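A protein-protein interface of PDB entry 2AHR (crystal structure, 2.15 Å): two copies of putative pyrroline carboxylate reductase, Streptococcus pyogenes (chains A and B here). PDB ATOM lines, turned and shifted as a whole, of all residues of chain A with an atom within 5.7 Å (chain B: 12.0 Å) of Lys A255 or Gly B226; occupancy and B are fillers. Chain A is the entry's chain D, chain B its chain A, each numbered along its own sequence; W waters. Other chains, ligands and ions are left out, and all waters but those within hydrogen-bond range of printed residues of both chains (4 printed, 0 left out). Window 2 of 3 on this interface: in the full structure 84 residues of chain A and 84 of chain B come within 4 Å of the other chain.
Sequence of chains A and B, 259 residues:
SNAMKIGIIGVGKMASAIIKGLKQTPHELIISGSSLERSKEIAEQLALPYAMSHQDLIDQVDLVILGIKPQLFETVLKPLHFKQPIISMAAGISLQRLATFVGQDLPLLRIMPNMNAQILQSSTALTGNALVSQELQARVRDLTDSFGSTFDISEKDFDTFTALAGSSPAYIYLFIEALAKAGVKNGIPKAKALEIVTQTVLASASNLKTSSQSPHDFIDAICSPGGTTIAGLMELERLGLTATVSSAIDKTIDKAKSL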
ATOM      1  N   GLN A  71      23.210  18.161 -20.917  1.00  0.00           N
ATOM      2  CA  GLN A  71      24.305  19.114 -20.751  1.00  0.00           C
ATOM      3  C   GLN A  71      25.616  18.482 -20.297  1.00  0.00           C
ATOM      4  O   GLN A  71      26.662  19.085 -20.472  1.00  0.00           O
ATOM      5  CB  GLN A  71      23.918  20.202 -19.748  1.00  0.00           C
ATOM      6  CG  GLN A  71      22.844  21.149 -20.253  1.00  0.00           C
ATOM      7  CD  GLN A  71      21.437  20.715 -19.901  1.00  0.00           C
ATOM      8  OE1 GLN A  71      21.208  19.618 -19.386  1.00  0.00           O
ATOM      9  NE2 GLN A  71      20.474  21.585 -20.188  1.00  0.00           N
ATOM     10  N   ASP A 250       5.846  24.164 -29.005  1.00  0.00           N
ATOM     11  CA  ASP A 250       6.865  24.710 -29.879  1.00  0.00           C
ATOM     12  C   ASP A 250       8.120  25.093 -29.076  1.00  0.00           C
ATOM     13  O   ASP A 250       9.242  24.811 -29.507  1.00  0.00           O
ATOM     14  CB  ASP A 250       6.331  25.929 -30.669  1.00  0.00           C
ATOM     15  CG  ASP A 250       5.476  25.535 -31.890  1.00  0.00           C
ATOM     16  OD1 ASP A 250       5.372  24.327 -32.243  1.00  0.00           O
ATOM     17  OD2 ASP A 250       4.894  26.459 -32.504  1.00  0.00           O
ATOM     18  N   LYS A 251       7.938  25.745 -27.929  1.00  0.00           N
ATOM     19  CA  LYS A 251       9.068  26.137 -27.079  1.00  0.00           C
ATOM     20  C   LYS A 251       9.810  24.946 -26.482  1.00  0.00           C
ATOM     21  O   LYS A 251      11.034  24.959 -26.364  1.00  0.00           O
ATOM     22  CB  LYS A 251       8.603  27.066 -25.968  1.00  0.00           C
ATOM     23  CG  LYS A 251       8.469  28.519 -26.437  1.00  0.00           C
ATOM     24  CD  LYS A 251       9.799  29.258 -26.264  1.00  0.00           C
ATOM     25  CE  LYS A 251       9.722  30.676 -26.826  1.00  0.00           C
ATOM     26  NZ  LYS A 251      10.885  31.513 -26.367  1.00  0.00           N
ATOM     27  N   THR A 252       9.066  23.918 -26.102  1.00  0.00           N
ATOM     28  CA  THR A 252       9.658  22.653 -25.616  1.00  0.00           C
ATOM     29  C   THR A 252      10.581  22.057 -26.691  1.00  0.00           C
ATOM     30  O   THR A 252      11.703  21.656 -26.418  1.00  0.00           O
ATOM     31  CB  THR A 252       8.561  21.661 -25.256  1.00  0.00           C
ATOM     32  OG1 THR A 252       7.637  22.296 -24.361  1.00  0.00           O
ATOM     33  CG2 THR A 252       9.139  20.383 -24.581  1.00  0.00           C
ATOM     34  N   ILE A 253      10.086  22.017 -27.920  1.00  0.00           N
ATOM     35  CA  ILE A 253      10.829  21.493 -29.065  1.00  0.00           C
ATOM     36  C   ILE A 253      12.031  22.376 -29.433  1.00  0.00           C
ATOM     37  O   ILE A 253      13.109  21.849 -29.672  1.00  0.00           O
ATOM     38  CB  ILE A 253       9.872  21.240 -30.271  1.00  0.00           C
ATOM     39  CG1 ILE A 253       8.881  20.104 -29.933  1.00  0.00           C
ATOM     40  CG2 ILE A 253      10.673  20.872 -31.533  1.00  0.00           C
ATOM     41  CD1 ILE A 253       7.682  20.020 -30.898  1.00  0.00           C
ATOM     42  N   ASP A 254      11.857  23.705 -29.469  1.00  0.00           N
ATOM     43  CA  ASP A 254      12.999  24.644 -29.641  1.00  0.00           C
ATOM     44  C   ASP A 254      14.153  24.336 -28.678  1.00  0.00           C
ATOM     45  O   ASP A 254      15.323  24.272 -29.075  1.00  0.00           O
ATOM     46  CB  ASP A 254      12.587  26.116 -29.426  1.00  0.00           C
ATOM     47  CG  ASP A 254      11.700  26.657 -30.537  1.00  0.00           C
ATOM     48  OD1 ASP A 254      11.654  26.049 -31.613  1.00  0.00           O
ATOM     49  OD2 ASP A 254      11.047  27.712 -30.349  1.00  0.00           O
ATOM     50  N   LYS A 255      13.815  24.161 -27.405  1.00  0.00           N
ATOM     51  CA  LYS A 255      14.805  23.827 -26.387  1.00  0.00           C
ATOM     52  C   LYS A 255      15.475  22.493 -26.684  1.00  0.00           C
ATOM     53  O   LYS A 255      16.701  22.355 -26.553  1.00  0.00           O
ATOM     54  CB  LYS A 255      14.179  23.802 -25.003  1.00  0.00           C
ATOM     55  CG  LYS A 255      15.195  23.521 -23.882  1.00  0.00           C
ATOM     56  CD  LYS A 255      16.165  24.706 -23.688  1.00  0.00           C
ATOM     57  CE  LYS A 255      17.316  24.262 -22.796  1.00  0.00           C
ATOM     58  NZ  LYS A 255      18.179  25.406 -22.429  1.00  0.00           N
ATOM     59  N   ALA A 256      14.689  21.508 -27.090  1.00  0.00           N
ATOM     60  CA  ALA A 256      15.268  20.196 -27.398  1.00  0.00           C
ATOM     61  C   ALA A 256      16.253  20.344 -28.561  1.00  0.00           C
ATOM     62  O   ALA A 256      17.369  19.837 -28.506  1.00  0.00           O
ATOM     63  CB  ALA A 256      14.168  19.176 -27.733  1.00  0.00           C
ATOM     64  N   LYS A 257      15.837  21.047 -29.611  1.00  0.00           N
ATOM     65  CA  LYS A 257      16.723  21.371 -30.731  1.00  0.00           C
ATOM     66  C   LYS A 257      18.036  22.041 -30.272  1.00  0.00           C
ATOM     67  O   LYS A 257      19.124  21.626 -30.699  1.00  0.00           O
ATOM     68  CB  LYS A 257      16.003  22.230 -31.779  1.00  0.00           C
ATOM     69  CG  LYS A 257      15.052  21.426 -32.672  1.00  0.00           C
ATOM     70  CD  LYS A 257      14.138  22.334 -33.501  1.00  0.00           C
ATOM     71  CE  LYS A 257      13.142  21.508 -34.342  1.00  0.00           C
ATOM     72  NZ  LYS A 257      12.018  22.344 -34.908  1.00  0.00           N
ATOM     73  N   SER A 258      17.955  23.035 -29.393  1.00  0.00           N
ATOM     74  CA  SER A 258      19.176  23.759 -29.015  1.00  0.00           C
ATOM     75  C   SER A 258      20.086  22.911 -28.120  1.00  0.00           C
ATOM     76  O   SER A 258      21.304  23.083 -28.136  1.00  0.00           O
ATOM     77  CB  SER A 258      18.865  25.104 -28.374  1.00  0.00           C
ATOM     78  OG  SER A 258      18.421  24.932 -27.054  1.00  0.00           O
ATOM     79  N   LEU A 259      19.520  21.970 -27.367  1.00  0.00           N
ATOM     80  CA  LEU A 259      20.368  21.077 -26.562  1.00  0.00           C
ATOM     81  C   LEU A 259      21.264  20.225 -27.472  1.00  0.00           C
ATOM     82  O   LEU A 259      20.895  19.879 -28.604  1.00  0.00           O
ATOM     83  CB  LEU A 259      19.543  20.172 -25.648  1.00  0.00           C
ATOM     84  CG  LEU A 259      18.767  20.806 -24.494  1.00  0.00           C
ATOM     85  CD1 LEU A 259      17.892  19.746 -23.825  1.00  0.00           C
ATOM     86  CD2 LEU A 259      19.700  21.492 -23.466  1.00  0.00           C
ATOM     87  OXT LEU A 259      22.385  19.882 -27.101  1.00  0.00           O
ATOM     88  N   ASN B 186       4.116  19.739 -35.797  1.00  0.00           N
ATOM     89  CA  ASN B 186       5.520  19.346 -35.734  1.00  0.00           C
ATOM     90  C   ASN B 186       5.843  17.929 -36.286  1.00  0.00           C
ATOM     91  O   ASN B 186       6.862  17.348 -35.931  1.00  0.00           O
ATOM     92  CB  ASN B 186       6.021  19.517 -34.291  1.00  0.00           C
ATOM     93  CG  ASN B 186       6.145  20.969 -33.898  1.00  0.00           C
ATOM     94  OD1 ASN B 186       7.122  21.616 -34.245  1.00  0.00           O
ATOM     95  ND2 ASN B 186       5.141  21.497 -33.181  1.00  0.00           N
ATOM     96  N   ILE B 219       5.242  18.477 -10.961  1.00  0.00           N
ATOM     97  CA  ILE B 219       5.890  19.450 -11.848  1.00  0.00           C
ATOM     98  C   ILE B 219       7.358  19.619 -11.489  1.00  0.00           C
ATOM     99  O   ILE B 219       8.211  19.614 -12.383  1.00  0.00           O
ATOM    100  CB  ILE B 219       5.123  20.783 -11.908  1.00  0.00           C
ATOM    101  CG1 ILE B 219       3.796  20.561 -12.639  1.00  0.00           C
ATOM    102  CG2 ILE B 219       5.961  21.872 -12.610  1.00  0.00           C
ATOM    103  CD1 ILE B 219       2.784  21.711 -12.528  1.00  0.00           C
ATOM    104  N   ASP B 220       7.664  19.734 -10.194  1.00  0.00           N
ATOM    105  CA  ASP B 220       9.060  19.862  -9.745  1.00  0.00           C
ATOM    106  C   ASP B 220       9.931  18.655 -10.124  1.00  0.00           C
ATOM    107  O   ASP B 220      11.116  18.813 -10.470  1.00  0.00           O
ATOM    108  CB  ASP B 220       9.155  20.068  -8.229  1.00  0.00           C
ATOM    109  CG  ASP B 220       8.880  21.505  -7.793  1.00  0.00           C
ATOM    110  OD1 ASP B 220       8.974  22.440  -8.627  1.00  0.00           O
ATOM    111  OD2 ASP B 220       8.582  21.687  -6.579  1.00  0.00           O
ATOM    112  N   ALA B 221       9.355  17.455 -10.026  1.00  0.00           N
ATOM    113  CA  ALA B 221      10.076  16.239 -10.379  1.00  0.00           C
ATOM    114  C   ALA B 221      10.341  16.180 -11.892  1.00  0.00           C
ATOM    115  O   ALA B 221      11.418  15.749 -12.324  1.00  0.00           O
ATOM    116  CB  ALA B 221       9.315  15.003  -9.901  1.00  0.00           C
ATOM    117  N   ILE B 222       9.372  16.640 -12.679  1.00  0.00           N
ATOM    118  CA  ILE B 222       9.446  16.569 -14.138  1.00  0.00           C
ATOM    119  C   ILE B 222      10.371  17.648 -14.775  1.00  0.00           C
ATOM    120  O   ILE B 222      11.007  17.402 -15.813  1.00  0.00           O
ATOM    121  CB  ILE B 222       8.021  16.594 -14.753  1.00  0.00           C
ATOM    122  CG1 ILE B 222       7.257  15.325 -14.360  1.00  0.00           C
ATOM    123  CG2 ILE B 222       8.061  16.726 -16.277  1.00  0.00           C
ATOM    124  CD1 ILE B 222       5.740  15.447 -14.445  1.00  0.00           C
ATOM    125  N   CYS B 223      10.459  18.826 -14.157  1.00  0.00           N
ATOM    126  CA  CYS B 223      11.244  19.913 -14.724  1.00  0.00           C
ATOM    127  C   CYS B 223      12.758  19.805 -14.454  1.00  0.00           C
ATOM    128  O   CYS B 223      13.259  20.397 -13.499  1.00  0.00           O
ATOM    129  CB  CYS B 223      10.697  21.272 -14.245  1.00  0.00           C
ATOM    130  SG  CYS B 223       9.127  21.725 -15.026  1.00  0.00           S
ATOM    131  N   SER B 224      13.484  19.077 -15.305  1.00  0.00           N
ATOM    132  CA  SER B 224      14.947  18.984 -15.190  1.00  0.00           C
ATOM    133  C   SER B 224      15.549  20.388 -15.334  1.00  0.00           C
ATOM    134  O   SER B 224      15.108  21.153 -16.198  1.00  0.00           O
ATOM    135  CB  SER B 224      15.519  18.082 -16.291  1.00  0.00           C
ATOM    136  OG  SER B 224      14.778  16.862 -16.448  1.00  0.00           O
ATOM    137  N   PRO B 225      16.565  20.724 -14.508  1.00  0.00           N
ATOM    138  CA  PRO B 225      17.211  22.040 -14.588  1.00  0.00           C
ATOM    139  C   PRO B 225      17.813  22.263 -15.980  1.00  0.00           C
ATOM    140  O   PRO B 225      18.510  21.381 -16.495  1.00  0.00           O
ATOM    141  CB  PRO B 225      18.325  21.966 -13.527  1.00  0.00           C
ATOM    142  CG  PRO B 225      17.888  20.843 -12.588  1.00  0.00           C
ATOM    143  CD  PRO B 225      17.176  19.861 -13.474  1.00  0.00           C
ATOM    144  N   GLY B 226      17.525  23.424 -16.578  1.00  0.00           N
ATOM    145  CA  GLY B 226      17.979  23.737 -17.945  1.00  0.00           C
ATOM    146  C   GLY B 226      17.333  22.859 -19.025  1.00  0.00           C
ATOM    147  O   GLY B 226      17.829  22.797 -20.129  1.00  0.00           O
ATOM    148  N   GLY B 227      16.222  22.198 -18.719  1.00  0.00           N
ATOM    149  CA  GLY B 227      15.613  21.235 -19.657  1.00  0.00           C
ATOM    150  C   GLY B 227      14.502  21.764 -20.549  1.00  0.00           C
ATOM    151  O   GLY B 227      14.256  22.996 -20.621  1.00  0.00           O
ATOM    152  N   THR B 228      13.832  20.832 -21.236  1.00  0.00           N
ATOM    153  CA  THR B 228      12.801  21.161 -22.216  1.00  0.00           C
ATOM    154  C   THR B 228      11.497  21.522 -21.518  1.00  0.00           C
ATOM    155  O   THR B 228      10.837  22.496 -21.890  1.00  0.00           O
ATOM    156  CB  THR B 228      12.549  19.993 -23.246  1.00  0.00           C
ATOM    157  OG1 THR B 228      12.077  18.834 -22.551  1.00  0.00           O
ATOM    158  CG2 THR B 228      13.824  19.597 -24.026  1.00  0.00           C
ATOM    159  N   THR B 229      11.118  20.728 -20.518  1.00  0.00           N
ATOM    160  CA  THR B 229       9.831  20.892 -19.835  1.00  0.00           C
ATOM    161  C   THR B 229       9.676  22.240 -19.160  1.00  0.00           C
ATOM    162  O   THR B 229       8.608  22.818 -19.223  1.00  0.00           O
ATOM    163  CB  THR B 229       9.576  19.784 -18.795  1.00  0.00           C
ATOM    164  OG1 THR B 229       9.735  18.503 -19.413  1.00  0.00           O
ATOM    165  CG2 THR B 229       8.153  19.893 -18.232  1.00  0.00           C
ATOM    166  N   ILE B 230      10.728  22.730 -18.504  1.00  0.00           N
ATOM    167  CA  ILE B 230      10.675  24.031 -17.840  1.00  0.00           C
ATOM    168  C   ILE B 230      10.589  25.168 -18.862  1.00  0.00           C
ATOM    169  O   ILE B 230       9.972  26.188 -18.582  1.00  0.00           O
ATOM    170  CB  ILE B 230      11.846  24.247 -16.820  1.00  0.00           C
ATOM    171  CG1 ILE B 230      11.691  25.553 -16.051  1.00  0.00           C
ATOM    172  CG2 ILE B 230      13.239  24.214 -17.490  1.00  0.00           C
ATOM    173  CD1 ILE B 230      10.506  25.577 -15.095  1.00  0.00           C
ATOM    174  N   ALA B 231      11.177  24.971 -20.044  1.00  0.00           N
ATOM    175  CA  ALA B 231      11.016  25.914 -21.155  1.00  0.00           C
ATOM    176  C   ALA B 231       9.557  25.974 -21.613  1.00  0.00           C
ATOM    177  O   ALA B 231       8.997  27.061 -21.789  1.00  0.00           O
ATOM    178  CB  ALA B 231      11.927  25.552 -22.317  1.00  0.00           C
ATOM    179  N   GLY B 232       8.931  24.812 -21.781  1.00  0.00           N
ATOM    180  CA  GLY B 232       7.524  24.797 -22.151  1.00  0.00           C
ATOM    181  C   GLY B 232       6.619  25.314 -21.045  1.00  0.00           C
ATOM    182  O   GLY B 232       5.627  25.997 -21.325  1.00  0.00           O
ATOM    183  N   LEU B 233       6.967  25.009 -19.784  1.00  0.00           N
ATOM    184  CA  LEU B 233       6.142  25.424 -18.643  1.00  0.00           C
ATOM    185  C   LEU B 233       6.105  26.944 -18.520  1.00  0.00           C
ATOM    186  O   LEU B 233       5.057  27.509 -18.245  1.00  0.00           O
ATOM    187  CB  LEU B 233       6.643  24.814 -17.337  1.00  0.00           C
ATOM    188  CG  LEU B 233       5.715  25.020 -16.138  1.00  0.00           C
ATOM    189  CD1 LEU B 233       4.611  23.945 -16.131  1.00  0.00           C
ATOM    190  CD2 LEU B 233       6.510  25.026 -14.804  1.00  0.00           C
ATOM    191  N   MET B 234       7.251  27.590 -18.716  1.00  0.00           N
ATOM    192  CA  MET B 234       7.329  29.050 -18.613  1.00  0.00           C
ATOM    193  C   MET B 234       6.667  29.743 -19.820  1.00  0.00           C
ATOM    194  O   MET B 234       6.275  30.916 -19.730  1.00  0.00           O
ATOM    195  CB  MET B 234       8.772  29.533 -18.411  1.00  0.00           C
ATOM    196  CG  MET B 234       9.401  29.107 -17.066  1.00  0.00           C
ATOM    197  SD  MET B 234       8.468  29.696 -15.590  1.00  0.00           S
ATOM    198  CE  MET B 234       7.790  28.192 -15.091  1.00  0.00           C
ATOM    199  N   GLU B 235       6.527  29.026 -20.934  1.00  0.00           N
ATOM    200  CA  GLU B 235       5.704  29.532 -22.040  1.00  0.00           C
ATOM    201  C   GLU B 235       4.214  29.508 -21.660  1.00  0.00           C
ATOM    202  O   GLU B 235       3.486  30.451 -21.963  1.00  0.00           O
ATOM    203  CB  GLU B 235       5.973  28.772 -23.363  1.00  0.00           C
ATOM    204  CG  GLU B 235       5.230  29.336 -24.623  1.00  0.00           C
ATOM    205  CD  GLU B 235       5.670  30.752 -25.070  1.00  0.00           C
ATOM    206  OE1 GLU B 235       6.419  31.449 -24.330  1.00  0.00           O
ATOM    207  OE2 GLU B 235       5.244  31.173 -26.182  1.00  0.00           O
HETATM  208  O   HOH W   1       9.231  20.810 -35.484  1.00  0.00           O
HETATM  209  O   HOH W   2       2.932  23.321 -32.095  1.00  0.00           O
HETATM  210  O   HOH W   3      18.550  19.186 -18.962  1.00  0.00           O
HETATM  211  O   HOH W   4      20.624  24.384 -20.823  1.00  0.00           O
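Of the 18 printed residues of chain B, 7 touch a printed residue of chain A. Printed residues of chain B that touch a printed residue of chain A: Asn B186, Gly B226, Gly B227, Thr B228, Ala B231, Gly B232 and Glu B235. Hydrophobic or aromatic side chains of chain B within 4 Å of the printed part of chain A: Ala B231. Hydrophobic or aromatic side chains of chain A that line the printed part of chain B: Ile A253 and Ala A256.
No position is printed for both chains. Of the 11 pairs that touch across the chains among the printed residues, none has its exchanged pair printed and touching as well.
ND2 of Asn B186 lies within hydrogen-bond range of OD1 of Asp A250 (3.0 Å). The side-chain amide nitrogen (NE2) of Gln A71 is in hydrogen-bond range of the backbone carbonyl oxygen (O) of Gly B226, at 2.9 Å. The backbone carbonyl oxygen (O) of Gly B226 sits close to the side-chain amino group (NZ) of Lys A255 (3.5 Å).
Among the printed residues, merely in contact across the chains: Lys A251 with Glu B235 (3.8 Å), Thr A252 with Thr B228 (3.7 Å), Thr A252 with Gly B232 (3.3 Å), Ile A253 with Asn B186 (3.5 Å), Lys A255 with Gly B227 (3.4 Å), Lys A255 with Thr B228 (3.8 Å), Lys A255 with Ala B231 (3.9 Å) and Ala A256 with Thr B228 (3.7 Å).
Water W1 lies within hydrogen-bond range of the side-chain amide oxygen (OD1) of Asn B186 (2.6 Å) and the side-chain amino group (NZ) of Lys A257 (3.2 Å). Water W2 bridges OD1 of Asp A250 (2.6 Å) and ND2 of Asn B186 (3.1 Å). Water W3 bridges OE1 of Gln A71 (2.7 Å) and O of Pro B225 (3.3 Å). Water W4 lies within hydrogen-bond range of the side-chain amide nitrogen of Gln A71 (2.9 Å), the side-chain amino group of Lys A255 (3.1 Å) and the backbone carbonyl oxygen of Gly B226 (3.3 Å).
The backbone carbonyl oxygen of Lys A255 lies within hydrogen-bond range of the side-chain hydroxyl of Ser A258 (3.1 Å).
Lys A255 touches four residues of chain B. Printed residues of chain A within 4 Å of Gly B226: Gln A71 and Lys A255. Thr A252 touches two residues of chain B. No residue of chain B comes within 4 Å of Asp A254. Ala A256 touches one residue of chain B. No residue of chain B comes within 4 Å of Lys A257. No residue of chain B comes within 4 Å of Ser A258. Printed residues of chain B within 4 Å of Lys A251: Glu B235. Printed residues of chain A within 4 Å of Gly B227: Lys A255. Printed residues of chain B within 4 Å of Asp A250: Asn B186. Of the printed residues of chain A, Asn B186 touches Asp A250 (3.0 Å) and Ile A253 (3.5 Å). Printed residues of chain A within 4 Å of Thr B228: Thr A252 (3.7 Å), Lys A255 (3.8 Å) and Ala A256 (3.7 Å). Ala B221 touches none of the printed residues of chain A. Asp B220 touches none of the printed residues of chain A. The nearest printed residue of chain A that does not touch Thr B228 is Leu A259 (4.1 Å).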
